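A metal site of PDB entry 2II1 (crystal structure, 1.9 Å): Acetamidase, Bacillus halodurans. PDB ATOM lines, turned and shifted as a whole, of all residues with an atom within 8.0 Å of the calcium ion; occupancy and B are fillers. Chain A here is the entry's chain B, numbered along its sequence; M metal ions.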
ATOM      1  N   ALA A 247      16.534  16.846  -7.616  1.00  0.00           N
ATOM      2  CA  ALA A 247      15.910  15.550  -7.234  1.00  0.00           C
ATOM      3  C   ALA A 247      15.125  14.931  -8.394  1.00  0.00           C
ATOM      4  O   ALA A 247      15.259  13.758  -8.722  1.00  0.00           O
ATOM      5  CB  ALA A 247      14.954  15.744  -6.027  1.00  0.00           C
ATOM      6  N   THR A 248      14.276  15.721  -9.015  1.00  0.00           N
ATOM      7  CA  THR A 248      13.447  15.216 -10.067  1.00  0.00           C
ATOM      8  C   THR A 248      14.285  14.843 -11.303  1.00  0.00           C
ATOM      9  O   THR A 248      13.999  13.825 -11.914  1.00  0.00           O
ATOM     10  CB  THR A 248      12.349  16.218 -10.442  1.00  0.00           C
ATOM     11  OG1 THR A 248      12.952  17.473 -10.778  1.00  0.00           O
ATOM     12  CG2 THR A 248      11.389  16.403  -9.301  1.00  0.00           C
ATOM     13  N   PHE A 249      15.292  15.652 -11.640  1.00  0.00           N
ATOM     14  CA  PHE A 249      16.294  15.313 -12.673  1.00  0.00           C
ATOM     15  C   PHE A 249      17.060  13.983 -12.400  1.00  0.00           C
ATOM     16  O   PHE A 249      17.174  13.114 -13.271  1.00  0.00           O
ATOM     17  CB  PHE A 249      17.289  16.478 -12.840  1.00  0.00           C
ATOM     18  CG  PHE A 249      18.502  16.147 -13.678  1.00  0.00           C
ATOM     19  CD1 PHE A 249      18.357  15.594 -14.949  1.00  0.00           C
ATOM     20  CD2 PHE A 249      19.780  16.398 -13.210  1.00  0.00           C
ATOM     21  CE1 PHE A 249      19.475  15.273 -15.734  1.00  0.00           C
ATOM     22  CE2 PHE A 249      20.903  16.090 -13.994  1.00  0.00           C
ATOM     23  CZ  PHE A 249      20.749  15.516 -15.255  1.00  0.00           C
ATOM     24  N   LEU A 250      17.583  13.855 -11.188  1.00  0.00           N
ATOM     25  CA  LEU A 250      18.328  12.674 -10.772  1.00  0.00           C
ATOM     26  C   LEU A 250      17.403  11.425 -10.658  1.00  0.00           C
ATOM     27  O   LEU A 250      17.808  10.324 -10.992  1.00  0.00           O
ATOM     28  CB  LEU A 250      19.078  13.036  -9.463  1.00  0.00           C
ATOM     29  CG  LEU A 250      20.109  12.181  -8.719  1.00  0.00           C
ATOM     30  CD1 LEU A 250      21.356  11.860  -9.556  1.00  0.00           C
ATOM     31  CD2 LEU A 250      20.495  12.937  -7.443  1.00  0.00           C
ATOM     32  N   ALA A 251      16.146  11.596 -10.251  1.00  0.00           N
ATOM     33  CA  ALA A 251      15.197  10.490 -10.282  1.00  0.00           C
ATOM     34  C   ALA A 251      14.887  10.144 -11.721  1.00  0.00           C
ATOM     35  O   ALA A 251      14.992   8.990 -12.142  1.00  0.00           O
ATOM     36  CB  ALA A 251      13.923  10.836  -9.524  1.00  0.00           C
ATOM     37  N   ASN A 252      14.480  11.155 -12.492  1.00  0.00           N
ATOM     38  CA  ASN A 252      14.080  10.954 -13.882  1.00  0.00           C
ATOM     39  C   ASN A 252      15.140  10.290 -14.766  1.00  0.00           C
ATOM     40  O   ASN A 252      14.809   9.444 -15.572  1.00  0.00           O
ATOM     41  CB  ASN A 252      13.630  12.277 -14.537  1.00  0.00           C
ATOM     42  CG  ASN A 252      12.283  12.783 -14.006  1.00  0.00           C
ATOM     43  OD1 ASN A 252      11.441  12.022 -13.559  1.00  0.00           O
ATOM     44  ND2 ASN A 252      12.078  14.099 -14.069  1.00  0.00           N
ATOM     45  N   ARG A 253      16.403  10.671 -14.602  1.00  0.00           N
ATOM     46  CA  ARG A 253      17.481  10.239 -15.511  1.00  0.00           C
ATOM     47  C   ARG A 253      18.327   9.065 -15.014  1.00  0.00           C
ATOM     48  O   ARG A 253      19.200   8.576 -15.750  1.00  0.00           O
ATOM     49  CB  ARG A 253      18.388  11.423 -15.860  1.00  0.00           C
ATOM     50  CG  ARG A 253      17.767  12.407 -16.864  1.00  0.00           C
ATOM     51  N   THR A 254      18.047   8.571 -13.807  1.00  0.00           N
ATOM     52  CA  THR A 254      18.826   7.532 -13.147  1.00  0.00           C
ATOM     53  C   THR A 254      17.940   6.388 -12.647  1.00  0.00           C
ATOM     54  O   THR A 254      16.703   6.534 -12.505  1.00  0.00           O
ATOM     55  CB  THR A 254      19.582   8.116 -11.897  1.00  0.00           C
ATOM     56  OG1 THR A 254      20.207   9.378 -12.230  1.00  0.00           O
ATOM     57  CG2 THR A 254      20.635   7.167 -11.402  1.00  0.00           C
ATOM     58  N   ALA A 255      18.589   5.280 -12.310  1.00  0.00           N
ATOM     59  CA  ALA A 255      17.962   4.140 -11.681  1.00  0.00           C
ATOM     60  C   ALA A 255      17.443   4.460 -10.279  1.00  0.00           C
ATOM     61  O   ALA A 255      16.737   3.665  -9.688  1.00  0.00           O
ATOM     62  CB  ALA A 255      18.942   2.995 -11.604  1.00  0.00           C
ATOM     63  N   LEU A 256      17.794   5.626  -9.753  1.00  0.00           N
ATOM     64  CA  LEU A 256      17.330   6.001  -8.437  1.00  0.00           C
ATOM     65  C   LEU A 256      15.849   6.326  -8.482  1.00  0.00           C
ATOM     66  O   LEU A 256      15.385   6.942  -9.445  1.00  0.00           O
ATOM     67  CB  LEU A 256      18.071   7.264  -7.957  1.00  0.00           C
ATOM     68  CG  LEU A 256      19.573   7.225  -7.791  1.00  0.00           C
ATOM     69  CD1 LEU A 256      19.993   8.551  -7.128  1.00  0.00           C
ATOM     70  CD2 LEU A 256      20.069   6.029  -6.957  1.00  0.00           C
ATOM     71  N   SER A 257      15.136   5.966  -7.421  1.00  0.00           N
ATOM     72  CA  SER A 257      13.797   6.483  -7.148  1.00  0.00           C
ATOM     73  C   SER A 257      13.888   7.903  -6.630  1.00  0.00           C
ATOM     74  O   SER A 257      14.978   8.390  -6.303  1.00  0.00           O
ATOM     75  CB  SER A 257      13.132   5.626  -6.091  1.00  0.00           C
ATOM     76  OG  SER A 257      13.882   5.724  -4.891  1.00  0.00           O
ATOM     77  N   ILE A 258      12.745   8.564  -6.531  1.00  0.00           N
ATOM     78  CA  ILE A 258      12.681   9.928  -5.994  1.00  0.00           C
ATOM     79  C   ILE A 258      13.089   9.924  -4.539  1.00  0.00           C
ATOM     80  O   ILE A 258      13.686  10.869  -4.050  1.00  0.00           O
ATOM     81  CB  ILE A 258      11.268  10.566  -6.187  1.00  0.00           C
ATOM     82  CG1 ILE A 258      11.304  12.080  -5.905  1.00  0.00           C
ATOM     83  CG2 ILE A 258      10.215   9.825  -5.366  1.00  0.00           C
ATOM     84  CD1 ILE A 258      12.270  12.877  -6.822  1.00  0.00           C
ATOM     85  N   GLU A 260      15.346   7.653  -3.260  1.00  0.00           N
ATOM     86  CA  GLU A 260      16.796   7.444  -3.267  1.00  0.00           C
ATOM     87  C   GLU A 260      17.547   8.703  -3.706  1.00  0.00           C
ATOM     88  O   GLU A 260      18.605   9.026  -3.172  1.00  0.00           O
ATOM     89  CB  GLU A 260      17.146   6.282  -4.180  1.00  0.00           C
ATOM     90  CG  GLU A 260      16.701   4.941  -3.631  1.00  0.00           C
ATOM     91  CD  GLU A 260      16.950   3.813  -4.582  1.00  0.00           C
ATOM     92  OE1 GLU A 260      16.706   3.991  -5.774  1.00  0.00           O
ATOM     93  OE2 GLU A 260      17.381   2.749  -4.118  1.00  0.00           O
ATOM     94  N   ALA A 261      16.976   9.429  -4.663  1.00  0.00           N
ATOM     95  CA  ALA A 261      17.498  10.749  -5.053  1.00  0.00           C
ATOM     96  C   ALA A 261      17.524  11.743  -3.862  1.00  0.00           C
ATOM     97  O   ALA A 261      18.530  12.406  -3.618  1.00  0.00           O
ATOM     98  CB  ALA A 261      16.687  11.306  -6.243  1.00  0.00           C
HETATM   99 CA    CA M   1      14.436   6.687 -11.579  1.00  0.00          CA
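O of Leu 250 is in hydrogen-bond range of OG1 of Thr 254 (2.9 Å).
The calcium ion is bound by O of Leu 256, O of Ala 251 and O of Thr 254.
Residues that only touch the calcium ion: Ala 255.
Of the 14 residues printed, 4 come within 4 Å of the calcium ion.
The nearest printed residue that does not touch the calcium ion is Ser 257 (4.3 Å).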
